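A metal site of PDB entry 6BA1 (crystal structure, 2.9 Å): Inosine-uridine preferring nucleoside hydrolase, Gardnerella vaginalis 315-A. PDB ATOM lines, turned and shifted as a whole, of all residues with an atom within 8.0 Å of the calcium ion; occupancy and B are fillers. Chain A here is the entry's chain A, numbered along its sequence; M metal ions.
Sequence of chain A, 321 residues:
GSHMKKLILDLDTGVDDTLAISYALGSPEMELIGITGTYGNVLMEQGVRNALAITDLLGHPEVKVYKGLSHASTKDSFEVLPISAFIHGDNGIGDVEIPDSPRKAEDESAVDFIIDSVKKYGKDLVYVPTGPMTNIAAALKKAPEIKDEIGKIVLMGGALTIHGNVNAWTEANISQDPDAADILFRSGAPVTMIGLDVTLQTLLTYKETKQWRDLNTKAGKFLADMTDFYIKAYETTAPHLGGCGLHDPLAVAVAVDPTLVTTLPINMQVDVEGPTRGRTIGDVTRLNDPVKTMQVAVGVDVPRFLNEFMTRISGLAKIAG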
ATOM      1  N   ASP A  10       2.557  10.504  27.375  1.00  0.00           N
ATOM      2  CA  ASP A  10       2.186   9.358  28.201  1.00  0.00           C
ATOM      3  C   ASP A  10       3.212   8.266  27.879  1.00  0.00           C
ATOM      4  O   ASP A  10       3.116   7.614  26.832  1.00  0.00           O
ATOM      5  CB  ASP A  10       0.753   8.908  27.881  1.00  0.00           C
ATOM      6  CG  ASP A  10       0.206   7.855  28.844  1.00  0.00           C
ATOM      7  OD1 ASP A  10      -0.737   8.203  29.578  1.00  0.00           O
ATOM      8  OD2 ASP A  10       0.650   6.692  28.818  1.00  0.00           O
ATOM      9  N   LEU A  11       4.196   8.083  28.764  1.00  0.00           N
ATOM     10  CA  LEU A  11       5.458   7.419  28.413  1.00  0.00           C
ATOM     11  C   LEU A  11       5.846   6.226  29.294  1.00  0.00           C
ATOM     12  O   LEU A  11       5.742   6.289  30.525  1.00  0.00           O
ATOM     13  CB  LEU A  11       6.596   8.428  28.450  1.00  0.00           C
ATOM     14  CG  LEU A  11       6.419   9.711  27.638  1.00  0.00           C
ATOM     15  CD1 LEU A  11       7.607  10.636  27.870  1.00  0.00           C
ATOM     16  CD2 LEU A  11       6.245   9.405  26.156  1.00  0.00           C
ATOM     17  N   ASP A  12       6.295   5.163  28.629  1.00  0.00           N
ATOM     18  CA  ASP A  12       6.952   4.022  29.278  1.00  0.00           C
ATOM     19  C   ASP A  12       8.468   4.203  29.119  1.00  0.00           C
ATOM     20  O   ASP A  12       9.120   3.495  28.376  1.00  0.00           O
ATOM     21  CB  ASP A  12       6.450   2.658  28.726  1.00  0.00           C
ATOM     22  CG  ASP A  12       6.659   2.462  27.185  1.00  0.00           C
ATOM     23  OD1 ASP A  12       6.812   3.440  26.412  1.00  0.00           O
ATOM     24  OD2 ASP A  12       6.651   1.291  26.756  1.00  0.00           O
ATOM     25  N   THR A  13       9.002   5.169  29.861  1.00  0.00           N
ATOM     26  CA  THR A  13      10.324   5.743  29.574  1.00  0.00           C
ATOM     27  C   THR A  13      11.501   4.837  29.993  1.00  0.00           C
ATOM     28  O   THR A  13      11.759   4.708  31.179  1.00  0.00           O
ATOM     29  CB  THR A  13      10.468   7.112  30.293  1.00  0.00           C
ATOM     30  OG1 THR A  13       9.189   7.776  30.331  1.00  0.00           O
ATOM     31  CG2 THR A  13      11.481   7.977  29.577  1.00  0.00           C
ATOM     32  N   GLY A  14      12.231   4.191  29.073  1.00  0.00           N
ATOM     33  CA  GLY A  14      12.017   4.168  27.606  1.00  0.00           C
ATOM     34  C   GLY A  14      13.033   4.986  26.839  1.00  0.00           C
ATOM     35  O   GLY A  14      13.157   6.183  27.080  1.00  0.00           O
ATOM     36  N   VAL A  15      13.729   4.359  25.895  1.00  0.00           N
ATOM     37  CA  VAL A  15      14.809   5.010  25.141  1.00  0.00           C
ATOM     38  C   VAL A  15      14.255   5.960  24.096  1.00  0.00           C
ATOM     39  O   VAL A  15      14.566   7.150  24.097  1.00  0.00           O
ATOM     40  CB  VAL A  15      15.781   4.009  24.479  1.00  0.00           C
ATOM     41  CG1 VAL A  15      16.861   4.745  23.694  1.00  0.00           C
ATOM     42  CG2 VAL A  15      16.405   3.091  25.522  1.00  0.00           C
ATOM     43  N   ASP A  16      13.445   5.412  23.187  1.00  0.00           N
ATOM     44  CA  ASP A  16      12.738   6.250  22.203  1.00  0.00           C
ATOM     45  C   ASP A  16      11.778   7.224  22.897  1.00  0.00           C
ATOM     46  O   ASP A  16      11.544   8.324  22.406  1.00  0.00           O
ATOM     47  CB  ASP A  16      12.020   5.435  21.085  1.00  0.00           C
ATOM     48  CG  ASP A  16      11.367   4.146  21.571  1.00  0.00           C
ATOM     49  OD1 ASP A  16      10.590   4.160  22.553  1.00  0.00           O
ATOM     50  OD2 ASP A  16      11.638   3.089  20.953  1.00  0.00           O
ATOM     51  N   ASP A  17      11.259   6.831  24.065  1.00  0.00           N
ATOM     52  CA  ASP A  17      10.398   7.703  24.858  1.00  0.00           C
ATOM     53  C   ASP A  17      11.104   8.981  25.321  1.00  0.00           C
ATOM     54  O   ASP A  17      10.474  10.044  25.330  1.00  0.00           O
ATOM     55  CB  ASP A  17       9.798   6.930  26.036  1.00  0.00           C
ATOM     56  CG  ASP A  17       8.809   5.851  25.581  1.00  0.00           C
ATOM     57  OD1 ASP A  17       9.244   4.759  25.154  1.00  0.00           O
ATOM     58  OD2 ASP A  17       7.587   6.094  25.656  1.00  0.00           O
ATOM     59  N   THR A  18      12.390   8.922  25.681  1.00  0.00           N
ATOM     60  CA  THR A  18      13.129  10.148  26.044  1.00  0.00           C
ATOM     61  C   THR A  18      13.472  10.994  24.834  1.00  0.00           C
ATOM     62  O   THR A  18      13.618  12.216  24.958  1.00  0.00           O
ATOM     63  CB  THR A  18      14.463   9.910  26.782  1.00  0.00           C
ATOM     64  OG1 THR A  18      15.435   9.380  25.886  1.00  0.00           O
ATOM     65  CG2 THR A  18      14.280   9.029  27.984  1.00  0.00           C
ATOM     66  N   THR A  38       3.574   5.390  32.268  1.00  0.00           N
ATOM     67  CA  THR A  38       2.955   4.082  32.094  1.00  0.00           C
ATOM     68  C   THR A  38       4.054   3.025  31.996  1.00  0.00           C
ATOM     69  O   THR A  38       5.215   3.312  32.312  1.00  0.00           O
ATOM     70  CB  THR A  38       1.955   4.088  30.888  1.00  0.00           C
ATOM     71  OG1 THR A  38       1.064   2.947  30.962  1.00  0.00           O
ATOM     72  CG2 THR A  38       2.683   4.079  29.549  1.00  0.00           C
ATOM     73  N   TYR A  39       3.701   1.806  31.556  1.00  0.00           N
ATOM     74  CA  TYR A  39       4.532   0.613  31.722  1.00  0.00           C
ATOM     75  C   TYR A  39       4.807  -0.034  30.363  1.00  0.00           C
ATOM     76  O   TYR A  39       4.151   0.297  29.378  1.00  0.00           O
ATOM     77  CB  TYR A  39       3.804  -0.393  32.621  1.00  0.00           C
ATOM     78  CG  TYR A  39       2.494  -0.893  32.022  1.00  0.00           C
ATOM     79  CD1 TYR A  39       2.441  -2.076  31.296  1.00  0.00           C
ATOM     80  CD2 TYR A  39       1.328  -0.141  32.143  1.00  0.00           C
ATOM     81  CE1 TYR A  39       1.261  -2.520  30.735  1.00  0.00           C
ATOM     82  CE2 TYR A  39       0.133  -0.571  31.579  1.00  0.00           C
ATOM     83  CZ  TYR A  39       0.105  -1.754  30.882  1.00  0.00           C
ATOM     84  OH  TYR A  39      -1.053  -2.191  30.298  1.00  0.00           O
ATOM     85  N   GLY A  40       5.757  -0.964  30.320  1.00  0.00           N
ATOM     86  CA  GLY A  40       6.039  -1.720  29.089  1.00  0.00           C
ATOM     87  C   GLY A  40       7.526  -1.916  28.882  1.00  0.00           C
ATOM     88  O   GLY A  40       8.066  -2.975  29.200  1.00  0.00           O
ATOM     89  N   ASN A  41       8.161  -0.893  28.315  1.00  0.00           N
ATOM     90  CA  ASN A  41       9.627  -0.870  28.153  1.00  0.00           C
ATOM     91  C   ASN A  41      10.292  -1.098  29.518  1.00  0.00           C
ATOM     92  O   ASN A  41      11.318  -1.780  29.623  1.00  0.00           O
ATOM     93  CB  ASN A  41      10.109   0.473  27.575  1.00  0.00           C
ATOM     94  CG  ASN A  41       9.675   0.689  26.127  1.00  0.00           C
ATOM     95  OD1 ASN A  41       9.138  -0.194  25.482  1.00  0.00           O
ATOM     96  ND2 ASN A  41       9.922   1.890  25.607  1.00  0.00           N
ATOM     97  N   VAL A  42       9.692  -0.504  30.546  1.00  0.00           N
ATOM     98  CA  VAL A  42      10.158  -0.652  31.906  1.00  0.00           C
ATOM     99  C   VAL A  42       8.971  -0.537  32.866  1.00  0.00           C
ATOM    100  O   VAL A  42       7.910  -0.017  32.488  1.00  0.00           O
ATOM    101  CB  VAL A  42      11.245   0.421  32.184  1.00  0.00           C
ATOM    102  CG1 VAL A  42      10.632   1.812  32.296  1.00  0.00           C
ATOM    103  CG2 VAL A  42      12.094   0.033  33.406  1.00  0.00           C
ATOM    104  N   HIS A  88      15.992  -1.666  25.709  1.00  0.00           N
ATOM    105  CA  HIS A  88      16.022  -0.426  26.492  1.00  0.00           C
ATOM    106  C   HIS A  88      16.886  -0.511  27.763  1.00  0.00           C
ATOM    107  O   HIS A  88      17.083   0.511  28.439  1.00  0.00           O
ATOM    108  CB  HIS A  88      14.596   0.032  26.846  1.00  0.00           C
ATOM    109  CG  HIS A  88      13.676   0.113  25.667  1.00  0.00           C
ATOM    110  ND1 HIS A  88      12.646  -0.772  25.467  1.00  0.00           N
ATOM    111  CD2 HIS A  88      13.656   0.956  24.603  1.00  0.00           C
ATOM    112  CE1 HIS A  88      12.018  -0.474  24.336  1.00  0.00           C
ATOM    113  NE2 HIS A  88      12.611   0.583  23.800  1.00  0.00           N
ATOM    114  N   PRO A 129       0.465   9.754  23.488  1.00  0.00           N
ATOM    115  CA  PRO A 129       0.872   8.544  24.201  1.00  0.00           C
ATOM    116  C   PRO A 129       1.717   7.606  23.374  1.00  0.00           C
ATOM    117  O   PRO A 129       1.258   7.115  22.368  1.00  0.00           O
ATOM    118  CB  PRO A 129      -0.474   7.889  24.518  1.00  0.00           C
ATOM    119  CG  PRO A 129      -1.342   8.297  23.386  1.00  0.00           C
ATOM    120  CD  PRO A 129      -0.908   9.654  22.969  1.00  0.00           C
ATOM    121  N   THR A 130       2.947   7.363  23.805  1.00  0.00           N
ATOM    122  CA  THR A 130       3.831   6.414  23.129  1.00  0.00           C
ATOM    123  C   THR A 130       4.196   5.227  24.038  1.00  0.00           C
ATOM    124  O   THR A 130       5.281   4.641  23.932  1.00  0.00           O
ATOM    125  CB  THR A 130       5.089   7.106  22.578  1.00  0.00           C
ATOM    126  OG1 THR A 130       6.053   7.262  23.629  1.00  0.00           O
ATOM    127  CG2 THR A 130       4.758   8.473  21.990  1.00  0.00           C
ATOM    128  N   GLY A 131       3.275   4.931  24.949  1.00  0.00           N
ATOM    129  CA  GLY A 131       3.263   3.666  25.651  1.00  0.00           C
ATOM    130  C   GLY A 131       1.885   3.068  25.427  1.00  0.00           C
ATOM    131  O   GLY A 131       1.123   3.555  24.592  1.00  0.00           O
ATOM    132  N   PRO A 132       1.549   2.007  26.179  1.00  0.00           N
ATOM    133  CA  PRO A 132       0.202   1.476  26.211  1.00  0.00           C
ATOM    134  C   PRO A 132      -0.876   2.528  26.438  1.00  0.00           C
ATOM    135  O   PRO A 132      -0.657   3.556  27.092  1.00  0.00           O
ATOM    136  CB  PRO A 132       0.248   0.513  27.382  1.00  0.00           C
ATOM    137  CG  PRO A 132       1.641  -0.015  27.336  1.00  0.00           C
ATOM    138  CD  PRO A 132       2.511   1.106  26.830  1.00  0.00           C
ATOM    139  N   MET A 156       1.728   6.700  19.252  1.00  0.00           N
ATOM    140  CA  MET A 156       2.654   5.806  18.556  1.00  0.00           C
ATOM    141  C   MET A 156       2.295   4.399  18.980  1.00  0.00           C
ATOM    142  O   MET A 156       2.261   4.087  20.164  1.00  0.00           O
ATOM    143  CB  MET A 156       4.120   6.155  18.854  1.00  0.00           C
ATOM    144  CG  MET A 156       5.089   4.981  19.053  1.00  0.00           C
ATOM    145  SD  MET A 156       5.118   3.698  17.784  1.00  0.00           S
ATOM    146  CE  MET A 156       5.966   2.364  18.658  1.00  0.00           C
ATOM    147  N   GLU A 171       1.623  -4.872  17.446  1.00  0.00           N
ATOM    148  CA  GLU A 171       2.764  -4.026  17.802  1.00  0.00           C
ATOM    149  C   GLU A 171       2.832  -3.829  19.324  1.00  0.00           C
ATOM    150  O   GLU A 171       1.805  -3.800  19.996  1.00  0.00           O
ATOM    151  CB  GLU A 171       2.655  -2.690  17.062  1.00  0.00           C
ATOM    152  CG  GLU A 171       3.747  -1.669  17.354  1.00  0.00           C
ATOM    153  CD  GLU A 171       3.569  -0.922  18.672  1.00  0.00           C
ATOM    154  OE1 GLU A 171       2.398  -0.753  19.119  1.00  0.00           O
ATOM    155  OE2 GLU A 171       4.593  -0.522  19.280  1.00  0.00           O
ATOM    156  N   ALA A 172       4.052  -3.673  19.842  1.00  0.00           N
ATOM    157  CA  ALA A 172       4.344  -3.628  21.292  1.00  0.00           C
ATOM    158  C   ALA A 172       3.356  -2.849  22.187  1.00  0.00           C
ATOM    159  O   ALA A 172       2.697  -3.449  23.031  1.00  0.00           O
ATOM    160  CB  ALA A 172       5.761  -3.106  21.511  1.00  0.00           C
ATOM    161  N   ASN A 173       3.269  -1.521  21.997  1.00  0.00           N
ATOM    162  CA  ASN A 173       2.389  -0.668  22.806  1.00  0.00           C
ATOM    163  C   ASN A 173       0.907  -1.116  22.784  1.00  0.00           C
ATOM    164  O   ASN A 173       0.197  -1.025  23.800  1.00  0.00           O
ATOM    165  CB  ASN A 173       2.527   0.812  22.386  1.00  0.00           C
ATOM    166  CG  ASN A 173       3.921   1.394  22.690  1.00  0.00           C
ATOM    167  OD1 ASN A 173       4.543   1.091  23.722  1.00  0.00           O
ATOM    168  ND2 ASN A 173       4.410   2.245  21.786  1.00  0.00           N
ATOM    169  N   TYR A 230      20.828   1.456  22.501  1.00  0.00           N
ATOM    170  CA  TYR A 230      19.632   1.158  21.708  1.00  0.00           C
ATOM    171  C   TYR A 230      19.975   0.665  20.296  1.00  0.00           C
ATOM    172  O   TYR A 230      19.313  -0.233  19.772  1.00  0.00           O
ATOM    173  CB  TYR A 230      18.757   2.407  21.663  1.00  0.00           C
ATOM    174  CG  TYR A 230      17.357   2.286  21.090  1.00  0.00           C
ATOM    175  CD1 TYR A 230      16.423   1.394  21.617  1.00  0.00           C
ATOM    176  CD2 TYR A 230      16.944   3.124  20.059  1.00  0.00           C
ATOM    177  CE1 TYR A 230      15.127   1.319  21.110  1.00  0.00           C
ATOM    178  CE2 TYR A 230      15.656   3.071  19.542  1.00  0.00           C
ATOM    179  CZ  TYR A 230      14.753   2.167  20.057  1.00  0.00           C
ATOM    180  OH  TYR A 230      13.489   2.109  19.527  1.00  0.00           O
ATOM    181  N   HIS A 247      10.624   5.734  16.671  1.00  0.00           N
ATOM    182  CA  HIS A 247       9.211   5.394  16.793  1.00  0.00           C
ATOM    183  C   HIS A 247       8.436   6.498  17.522  1.00  0.00           C
ATOM    184  O   HIS A 247       7.623   7.197  16.919  1.00  0.00           O
ATOM    185  CB  HIS A 247       9.026   4.049  17.510  1.00  0.00           C
ATOM    186  CG  HIS A 247       9.723   2.901  16.864  1.00  0.00           C
ATOM    187  ND1 HIS A 247       9.043   1.930  16.157  1.00  0.00           N
ATOM    188  CD2 HIS A 247      11.044   2.549  16.832  1.00  0.00           C
ATOM    189  CE1 HIS A 247       9.904   1.028  15.703  1.00  0.00           C
ATOM    190  NE2 HIS A 247      11.120   1.398  16.089  1.00  0.00           N
ATOM    191  N   ASP A 248       8.734   6.675  18.800  1.00  0.00           N
ATOM    192  CA  ASP A 248       7.979   7.554  19.677  1.00  0.00           C
ATOM    193  C   ASP A 248       8.154   9.059  19.362  1.00  0.00           C
ATOM    194  O   ASP A 248       7.192   9.821  19.461  1.00  0.00           O
ATOM    195  CB  ASP A 248       8.303   7.270  21.160  1.00  0.00           C
ATOM    196  CG  ASP A 248       8.047   5.790  21.544  1.00  0.00           C
ATOM    197  OD1 ASP A 248       8.150   4.873  20.673  1.00  0.00           O
ATOM    198  OD2 ASP A 248       7.741   5.511  22.729  1.00  0.00           O
HETATM  199 CA    CA M   1       7.520   3.324  23.961  1.00  0.00          CA
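The calcium ion is bound by OD2 of Asp 248, OD1 of Asp 17, OD1 of Asp 12 and O of Thr 130.
The calcium ion has four donor atoms within binding distance.
The side-chain carboxylate of Asp 17 lies close to the side-chain amide nitrogen of Asn 41 (3.0 Å).
OD2 of Asp 12 lies within hydrogen-bond range of N of Asn 41 (3.1 Å).
O of Thr 130 sits close to ND2 of Asn 173, at 3.3 Å.
N of Thr 130 sits at hydrogen-bond distance from O of Asp 10 (3.0 Å).
The side-chain amide nitrogen (ND2) of Asn 41 sits close to a ring nitrogen (NE2) of His 88 (3.5 Å).
OD2 of Asp 16 sits at hydrogen-bond distance from OH of Tyr 230.
The backbone carbonyl oxygen (O) of Met 156 lies within hydrogen-bond range of the side-chain amide nitrogen (ND2) of Asn 173, 3.3 Å away.
The side-chain carboxylate of Glu 171 sits at hydrogen-bond distance from the backbone NH of Asn 173 (3.1 Å).
OD1 of Asp 16 touches the calcium ion (3.5 Å).
Asn 41 touches the calcium ion.
Asn 173 touches the calcium ion (OD1 to CA, 3.7 Å).
Within 4 Å of the calcium ion: Asp 12, Asp 16, Asp 17, Asn 41, Thr 130, Asn 173 and Asp 248.
Along chain A the residues within 4 Å of the calcium ion span positions 12 to 248.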
